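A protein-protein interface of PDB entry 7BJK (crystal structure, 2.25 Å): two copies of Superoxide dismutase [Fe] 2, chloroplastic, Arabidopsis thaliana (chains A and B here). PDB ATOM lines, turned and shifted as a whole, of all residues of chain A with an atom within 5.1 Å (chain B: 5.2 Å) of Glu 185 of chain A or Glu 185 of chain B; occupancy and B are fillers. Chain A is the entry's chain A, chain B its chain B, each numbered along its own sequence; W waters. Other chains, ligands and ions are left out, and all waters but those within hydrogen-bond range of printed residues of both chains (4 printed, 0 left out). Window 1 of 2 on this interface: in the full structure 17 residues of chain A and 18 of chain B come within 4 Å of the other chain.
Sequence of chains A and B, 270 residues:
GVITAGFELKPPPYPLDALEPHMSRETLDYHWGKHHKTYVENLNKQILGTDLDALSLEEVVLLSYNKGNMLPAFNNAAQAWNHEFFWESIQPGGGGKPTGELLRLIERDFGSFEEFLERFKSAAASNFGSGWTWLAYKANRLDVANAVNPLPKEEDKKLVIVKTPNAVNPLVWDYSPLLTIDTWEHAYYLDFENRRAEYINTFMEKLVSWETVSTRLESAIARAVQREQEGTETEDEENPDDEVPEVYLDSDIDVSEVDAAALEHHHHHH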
ATOM      1  N   HIS A  35     -21.165   5.263  12.007  1.00  0.00           N
ATOM      2  CA  HIS A  35     -20.408   4.715  10.882  1.00  0.00           C
ATOM      3  C   HIS A  35     -21.306   4.469   9.677  1.00  0.00           C
ATOM      4  O   HIS A  35     -21.001   4.911   8.561  1.00  0.00           O
ATOM      5  CB  HIS A  35     -19.699   3.424  11.279  1.00  0.00           C
ATOM      6  CG  HIS A  35     -18.329   3.642  11.831  1.00  0.00           C
ATOM      7  ND1 HIS A  35     -17.275   4.068  11.052  1.00  0.00           N
ATOM      8  CD2 HIS A  35     -17.838   3.504  13.087  1.00  0.00           C
ATOM      9  CE1 HIS A  35     -16.192   4.179  11.803  1.00  0.00           C
ATOM     10  NE2 HIS A  35     -16.509   3.842  13.041  1.00  0.00           N
ATOM     11  N   SER A 130      -9.336  -4.920   8.662  1.00  0.00           N
ATOM     12  CA  SER A 130     -10.750  -4.590   8.512  1.00  0.00           C
ATOM     13  C   SER A 130     -11.410  -5.459   7.440  1.00  0.00           C
ATOM     14  O   SER A 130     -10.837  -5.671   6.362  1.00  0.00           O
ATOM     15  CB  SER A 130     -10.906  -3.112   8.129  1.00  0.00           C
ATOM     16  OG  SER A 130     -10.435  -2.250   9.143  1.00  0.00           O
ATOM     17  N   THR A 183     -16.260  -7.555  10.810  1.00  0.00           N
ATOM     18  CA  THR A 183     -15.128  -7.692  11.727  1.00  0.00           C
ATOM     19  C   THR A 183     -14.198  -6.486  11.664  1.00  0.00           C
ATOM     20  O   THR A 183     -13.057  -6.552  12.145  1.00  0.00           O
ATOM     21  CB  THR A 183     -14.351  -9.004  11.514  1.00  0.00           C
ATOM     22  OG1 THR A 183     -13.890  -9.130  10.159  1.00  0.00           O
ATOM     23  CG2 THR A 183     -15.229 -10.207  11.899  1.00  0.00           C
ATOM     24  N   TRP A 184     -14.672  -5.379  11.091  1.00  0.00           N
ATOM     25  CA  TRP A 184     -14.106  -4.072  11.402  1.00  0.00           C
ATOM     26  C   TRP A 184     -14.091  -3.858  12.914  1.00  0.00           C
ATOM     27  O   TRP A 184     -15.050  -4.200  13.611  1.00  0.00           O
ATOM     28  CB  TRP A 184     -14.946  -2.969  10.728  1.00  0.00           C
ATOM     29  CG  TRP A 184     -14.700  -2.810   9.270  1.00  0.00           C
ATOM     30  CD1 TRP A 184     -14.924  -3.735   8.285  1.00  0.00           C
ATOM     31  CD2 TRP A 184     -14.191  -1.646   8.618  1.00  0.00           C
ATOM     32  NE1 TRP A 184     -14.569  -3.217   7.061  1.00  0.00           N
ATOM     33  CE2 TRP A 184     -14.119  -1.936   7.242  1.00  0.00           C
ATOM     34  CE3 TRP A 184     -13.780  -0.386   9.065  1.00  0.00           C
ATOM     35  CZ2 TRP A 184     -13.649  -1.015   6.318  1.00  0.00           C
ATOM     36  CZ3 TRP A 184     -13.330   0.533   8.137  1.00  0.00           C
ATOM     37  CH2 TRP A 184     -13.267   0.216   6.782  1.00  0.00           C
ATOM     38  N   GLU A 185     -13.007  -3.262  13.426  1.00  0.00           N
ATOM     39  CA  GLU A 185     -12.901  -3.102  14.877  1.00  0.00           C
ATOM     40  C   GLU A 185     -14.080  -2.324  15.443  1.00  0.00           C
ATOM     41  O   GLU A 185     -14.546  -2.623  16.554  1.00  0.00           O
ATOM     42  CB  GLU A 185     -11.583  -2.424  15.256  1.00  0.00           C
ATOM     43  CG  GLU A 185     -10.321  -3.218  14.833  1.00  0.00           C
ATOM     44  CD  GLU A 185      -9.018  -2.530  15.244  1.00  0.00           C
ATOM     45  OE1 GLU A 185      -8.853  -1.339  14.899  1.00  0.00           O
ATOM     46  OE2 GLU A 185      -8.160  -3.183  15.916  1.00  0.00           O
ATOM     47  N   HIS A 186     -14.608  -1.356  14.682  1.00  0.00           N
ATOM     48  CA  HIS A 186     -15.700  -0.557  15.216  1.00  0.00           C
ATOM     49  C   HIS A 186     -16.908  -1.414  15.516  1.00  0.00           C
ATOM     50  O   HIS A 186     -17.768  -1.006  16.303  1.00  0.00           O
ATOM     51  CB  HIS A 186     -16.063   0.590  14.256  1.00  0.00           C
ATOM     52  CG  HIS A 186     -16.666   0.150  12.958  1.00  0.00           C
ATOM     53  ND1 HIS A 186     -16.161   0.545  11.736  1.00  0.00           N
ATOM     54  CD2 HIS A 186     -17.748  -0.619  12.689  1.00  0.00           C
ATOM     55  CE1 HIS A 186     -16.902   0.027  10.771  1.00  0.00           C
ATOM     56  NE2 HIS A 186     -17.871  -0.681  11.323  1.00  0.00           N
ATOM     57  N   ALA A 187     -16.972  -2.610  14.932  1.00  0.00           N
ATOM     58  CA  ALA A 187     -18.153  -3.439  15.110  1.00  0.00           C
ATOM     59  C   ALA A 187     -18.203  -4.098  16.473  1.00  0.00           C
ATOM     60  O   ALA A 187     -19.288  -4.520  16.883  1.00  0.00           O
ATOM     61  CB  ALA A 187     -18.242  -4.510  14.024  1.00  0.00           C
ATOM     62  N   TYR A 188     -17.070  -4.200  17.191  1.00  0.00           N
ATOM     63  CA  TYR A 188     -17.099  -4.910  18.463  1.00  0.00           C
ATOM     64  C   TYR A 188     -16.269  -4.293  19.587  1.00  0.00           C
ATOM     65  O   TYR A 188     -16.278  -4.850  20.696  1.00  0.00           O
ATOM     66  CB  TYR A 188     -16.674  -6.372  18.267  1.00  0.00           C
ATOM     67  CG  TYR A 188     -15.305  -6.567  17.650  1.00  0.00           C
ATOM     68  CD1 TYR A 188     -15.137  -6.566  16.278  1.00  0.00           C
ATOM     69  CD2 TYR A 188     -14.180  -6.773  18.440  1.00  0.00           C
ATOM     70  CE1 TYR A 188     -13.885  -6.751  15.700  1.00  0.00           C
ATOM     71  CE2 TYR A 188     -12.931  -6.968  17.868  1.00  0.00           C
ATOM     72  CZ  TYR A 188     -12.791  -6.954  16.497  1.00  0.00           C
ATOM     73  OH  TYR A 188     -11.550  -7.131  15.909  1.00  0.00           O
ATOM     74  N   TYR A 189     -15.592  -3.156  19.377  1.00  0.00           N
ATOM     75  CA  TYR A 189     -14.825  -2.569  20.483  1.00  0.00           C
ATOM     76  C   TYR A 189     -15.695  -2.327  21.714  1.00  0.00           C
ATOM     77  O   TYR A 189     -15.318  -2.685  22.836  1.00  0.00           O
ATOM     78  CB  TYR A 189     -14.161  -1.251  20.087  1.00  0.00           C
ATOM     79  CG  TYR A 189     -13.621  -0.624  21.333  1.00  0.00           C
ATOM     80  CD1 TYR A 189     -12.514  -1.169  21.959  1.00  0.00           C
ATOM     81  CD2 TYR A 189     -14.267   0.444  21.945  1.00  0.00           C
ATOM     82  CE1 TYR A 189     -12.032  -0.652  23.147  1.00  0.00           C
ATOM     83  CE2 TYR A 189     -13.797   0.975  23.129  1.00  0.00           C
ATOM     84  CZ  TYR A 189     -12.674   0.421  23.733  1.00  0.00           C
ATOM     85  OH  TYR A 189     -12.193   0.947  24.914  1.00  0.00           O
ATOM     86  N   HIS B  35      -3.466  -3.955  22.464  1.00  0.00           N
ATOM     87  CA  HIS B  35      -3.208  -4.284  21.064  1.00  0.00           C
ATOM     88  C   HIS B  35      -1.729  -4.559  20.812  1.00  0.00           C
ATOM     89  O   HIS B  35      -1.372  -5.600  20.245  1.00  0.00           O
ATOM     90  CB  HIS B  35      -3.721  -3.176  20.147  1.00  0.00           C
ATOM     91  CG  HIS B  35      -5.148  -3.366  19.749  1.00  0.00           C
ATOM     92  ND1 HIS B  35      -5.539  -4.300  18.810  1.00  0.00           N
ATOM     93  CD2 HIS B  35      -6.284  -2.775  20.189  1.00  0.00           C
ATOM     94  CE1 HIS B  35      -6.853  -4.268  18.684  1.00  0.00           C
ATOM     95  NE2 HIS B  35      -7.328  -3.342  19.499  1.00  0.00           N
ATOM     96  N   SER B 130      -7.952  -0.564   7.567  1.00  0.00           N
ATOM     97  CA  SER B 130      -6.827  -0.578   8.501  1.00  0.00           C
ATOM     98  C   SER B 130      -5.514  -0.361   7.765  1.00  0.00           C
ATOM     99  O   SER B 130      -5.278  -0.939   6.696  1.00  0.00           O
ATOM    100  CB  SER B 130      -6.768  -1.900   9.268  1.00  0.00           C
ATOM    101  OG  SER B 130      -7.883  -2.024  10.121  1.00  0.00           O
ATOM    102  N   THR B 183      -3.426   4.354  11.460  1.00  0.00           N
ATOM    103  CA  THR B 183      -4.832   4.676  11.221  1.00  0.00           C
ATOM    104  C   THR B 183      -5.746   3.459  11.311  1.00  0.00           C
ATOM    105  O   THR B 183      -6.826   3.468  10.719  1.00  0.00           O
ATOM    106  CB  THR B 183      -5.042   5.395   9.883  1.00  0.00           C
ATOM    107  OG1 THR B 183      -4.421   4.665   8.813  1.00  0.00           O
ATOM    108  CG2 THR B 183      -4.473   6.806   9.955  1.00  0.00           C
ATOM    109  N   TRP B 184      -5.338   2.414  12.031  1.00  0.00           N
ATOM    110  CA  TRP B 184      -6.298   1.422  12.500  1.00  0.00           C
ATOM    111  C   TRP B 184      -7.302   2.118  13.403  1.00  0.00           C
ATOM    112  O   TRP B 184      -6.941   3.031  14.150  1.00  0.00           O
ATOM    113  CB  TRP B 184      -5.600   0.289  13.285  1.00  0.00           C
ATOM    114  CG  TRP B 184      -4.878  -0.708  12.451  1.00  0.00           C
ATOM    115  CD1 TRP B 184      -3.844  -0.462  11.599  1.00  0.00           C
ATOM    116  CD2 TRP B 184      -5.103  -2.131  12.408  1.00  0.00           C
ATOM    117  NE1 TRP B 184      -3.430  -1.630  11.007  1.00  0.00           N
ATOM    118  CE2 TRP B 184      -4.177  -2.669  11.496  1.00  0.00           C
ATOM    119  CE3 TRP B 184      -5.986  -2.997  13.067  1.00  0.00           C
ATOM    120  CZ2 TRP B 184      -4.118  -4.036  11.207  1.00  0.00           C
ATOM    121  CZ3 TRP B 184      -5.917  -4.358  12.791  1.00  0.00           C
ATOM    122  CH2 TRP B 184      -5.008  -4.859  11.853  1.00  0.00           C
ATOM    123  N   GLU B 185      -8.565   1.681  13.342  1.00  0.00           N
ATOM    124  CA  GLU B 185      -9.603   2.324  14.149  1.00  0.00           C
ATOM    125  C   GLU B 185      -9.248   2.337  15.634  1.00  0.00           C
ATOM    126  O   GLU B 185      -9.637   3.269  16.351  1.00  0.00           O
ATOM    127  CB  GLU B 185     -10.956   1.637  13.921  1.00  0.00           C
ATOM    128  CG  GLU B 185     -11.583   1.981  12.568  1.00  0.00           C
ATOM    129  CD  GLU B 185     -12.943   1.310  12.320  1.00  0.00           C
ATOM    130  OE1 GLU B 185     -13.101   0.088  12.595  1.00  0.00           O
ATOM    131  OE2 GLU B 185     -13.861   2.014  11.829  1.00  0.00           O
ATOM    132  N   HIS B 186      -8.494   1.333  16.113  1.00  0.00           N
ATOM    133  CA  HIS B 186      -8.160   1.286  17.533  1.00  0.00           C
ATOM    134  C   HIS B 186      -7.201   2.405  17.921  1.00  0.00           C
ATOM    135  O   HIS B 186      -7.100   2.746  19.102  1.00  0.00           O
ATOM    136  CB  HIS B 186      -7.591  -0.101  17.916  1.00  0.00           C
ATOM    137  CG  HIS B 186      -6.220  -0.391  17.366  1.00  0.00           C
ATOM    138  ND1 HIS B 186      -5.941  -1.518  16.616  1.00  0.00           N
ATOM    139  CD2 HIS B 186      -5.044   0.282  17.482  1.00  0.00           C
ATOM    140  CE1 HIS B 186      -4.660  -1.511  16.272  1.00  0.00           C
ATOM    141  NE2 HIS B 186      -4.091  -0.439  16.796  1.00  0.00           N
ATOM    142  N   ALA B 187      -6.508   2.996  16.952  1.00  0.00           N
ATOM    143  CA  ALA B 187      -5.586   4.078  17.258  1.00  0.00           C
ATOM    144  C   ALA B 187      -6.298   5.329  17.738  1.00  0.00           C
ATOM    145  O   ALA B 187      -5.666   6.176  18.381  1.00  0.00           O
ATOM    146  CB  ALA B 187      -4.753   4.442  16.029  1.00  0.00           C
ATOM    147  N   TYR B 188      -7.587   5.493  17.422  1.00  0.00           N
ATOM    148  CA  TYR B 188      -8.192   6.788  17.704  1.00  0.00           C
ATOM    149  C   TYR B 188      -9.652   6.763  18.131  1.00  0.00           C
ATOM    150  O   TYR B 188     -10.204   7.838  18.362  1.00  0.00           O
ATOM    151  CB  TYR B 188      -8.033   7.694  16.490  1.00  0.00           C
ATOM    152  CG  TYR B 188      -8.679   7.190  15.206  1.00  0.00           C
ATOM    153  CD1 TYR B 188      -8.003   6.316  14.351  1.00  0.00           C
ATOM    154  CD2 TYR B 188      -9.949   7.617  14.835  1.00  0.00           C
ATOM    155  CE1 TYR B 188      -8.581   5.872  13.175  1.00  0.00           C
ATOM    156  CE2 TYR B 188     -10.537   7.187  13.658  1.00  0.00           C
ATOM    157  CZ  TYR B 188      -9.853   6.318  12.832  1.00  0.00           C
ATOM    158  OH  TYR B 188     -10.450   5.894  11.658  1.00  0.00           O
ATOM    159  N   TYR B 189     -10.292   5.595  18.273  1.00  0.00           N
ATOM    160  CA  TYR B 189     -11.679   5.599  18.730  1.00  0.00           C
ATOM    161  C   TYR B 189     -11.820   6.315  20.070  1.00  0.00           C
ATOM    162  O   TYR B 189     -12.728   7.127  20.255  1.00  0.00           O
ATOM    163  CB  TYR B 189     -12.255   4.181  18.851  1.00  0.00           C
ATOM    164  CG  TYR B 189     -13.588   4.291  19.565  1.00  0.00           C
ATOM    165  CD1 TYR B 189     -14.705   4.786  18.901  1.00  0.00           C
ATOM    166  CD2 TYR B 189     -13.713   3.990  20.915  1.00  0.00           C
ATOM    167  CE1 TYR B 189     -15.926   4.969  19.562  1.00  0.00           C
ATOM    168  CE2 TYR B 189     -14.924   4.164  21.584  1.00  0.00           C
ATOM    169  CZ  TYR B 189     -16.029   4.653  20.896  1.00  0.00           C
ATOM    170  OH  TYR B 189     -17.230   4.818  21.546  1.00  0.00           O
HETATM  171  O   HOH W   1     -13.368   4.890  13.106  1.00  0.00           O
HETATM  172  O   HOH W   2      -8.025  -3.338   6.556  1.00  0.00           O
HETATM  173  O   HOH W   3      -8.889  -0.976  12.238  1.00  0.00           O
HETATM  174  O   HOH W   4     -11.365  -1.753  11.554  1.00  0.00           O
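Water W3 lies within hydrogen-bond range of the side-chain hydroxyl (OG) of Ser 130 of chain B (2.6 Å), the side-chain carboxylate (OE1) of Glu 185 of chain A (2.7 Å) and the backbone NH (N) of Glu 185 of chain B (2.9 Å).
Water W4 lies within hydrogen-bond range of the side-chain hydroxyl (OG) of Ser 130 of chain A (2.6 Å), the side-chain carboxylate (OE1) of Glu 185 of chain B (2.7 Å) and the backbone NH (N) of Glu 185 of chain A (2.9 Å).
Water W2 lies within hydrogen-bond range of N of Ser 130 of chain A (2.9 Å) and N of Ser 130 of chain B (3.0 Å).
Water W1 lies within hydrogen-bond range of OE2 of Glu 185 of chain B (3.2 Å), NE2 of His 35 of chain A (3.3 Å) and OH of Tyr 188 of chain B (3.4 Å).
His 35 of chain A touches Glu 185 of chain B, and with the chains exchanged Glu 185 of chain A touches His 35 of chain B.
Ser 130 of chain A touches its own counterpart, Ser 130 of chain B.
Trp 184 of chain A touches Glu 185 of chain B, and with the chains exchanged Glu 185 of chain A touches Trp 184 of chain B.
Tyr 189 of chain A touches its own counterpart, Tyr 189 of chain B.
Positions printed for both chains: 35, 130, 183, 184, 185, 186, 187, 188 and 189.
The side-chain hydroxyl (OG) of Ser 130 of chain A lies within hydrogen-bond range of the side-chain hydroxyl (OG) of Ser 130 of chain B (2.7 Å).
A ring nitrogen (NE2) of His 35 of chain A lies close to the side-chain carboxylate of Glu 185 of chain B, 3.4 Å away.
OE1 of Glu 185 of chain A sits at hydrogen-bond distance from N of Glu 185 of chain B (3.4 Å).
The side-chain carboxylate (OE2) of Glu 185 of chain A sits at hydrogen-bond distance from a ring nitrogen (ND1) of His 186 of chain B, at 2.9 Å.
A ring nitrogen (ND1) of His 186 of chain A sits at hydrogen-bond distance from the side-chain carboxylate (OE2) of Glu 185 of chain B (2.7 Å).
Of the 9 printed residues of chain A, 6 touch a printed residue of chain B.
Printed residues of chain A that touch a printed residue of chain B: His 35, Ser 130, Trp 184, Glu 185, His 186 and Tyr 189.
Hydrophobic or aromatic side chains of chain A that line the printed part of chain B: His 35, Trp 184, His 186 and Tyr 189.
Hydrophobic or aromatic side chains of chain B that line the printed part of chain A: His 35, Trp 184, His 186 and Tyr 189.
Among the printed residues, 9 pairs touch across the chains.
Among the printed residues, no Asp or Glu carboxylate lies within 4 Å of a Lys or Arg side-chain nitrogen of the other chain.
Among the printed residues, merely in contact across the chains: Trp 184 of chain A with Glu 185 of chain B (3.6 Å), Glu 185 of chain A with His 35 of chain B (3.2 Å), Glu 185 of chain A with Trp 184 of chain B (3.6 Å) and Tyr 189 of chain A with Tyr 189 of chain B (3.7 Å).
Printed residues of chain B within 4 Å of His 35 of chain A: Glu 185 (3.2 Å).
Glu 185 of chain A touches just these residues of chain B: His 35 (3.2 Å), Trp 184 (3.6 Å), Glu 185 (3.4 Å) and His 186 (2.9 Å).
Of the printed residues of chain A, Ser 130 of chain B touches Ser 130 (2.7 Å).
Of the printed residues of chain A, Trp 184 of chain B touches Glu 185.
Of the printed residues of chain A, Tyr 189 of chain B touches Tyr 189.
The nearest printed residue of chain A that does not touch Tyr 189 of chain B is His 35 of chain A (6.2 Å).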
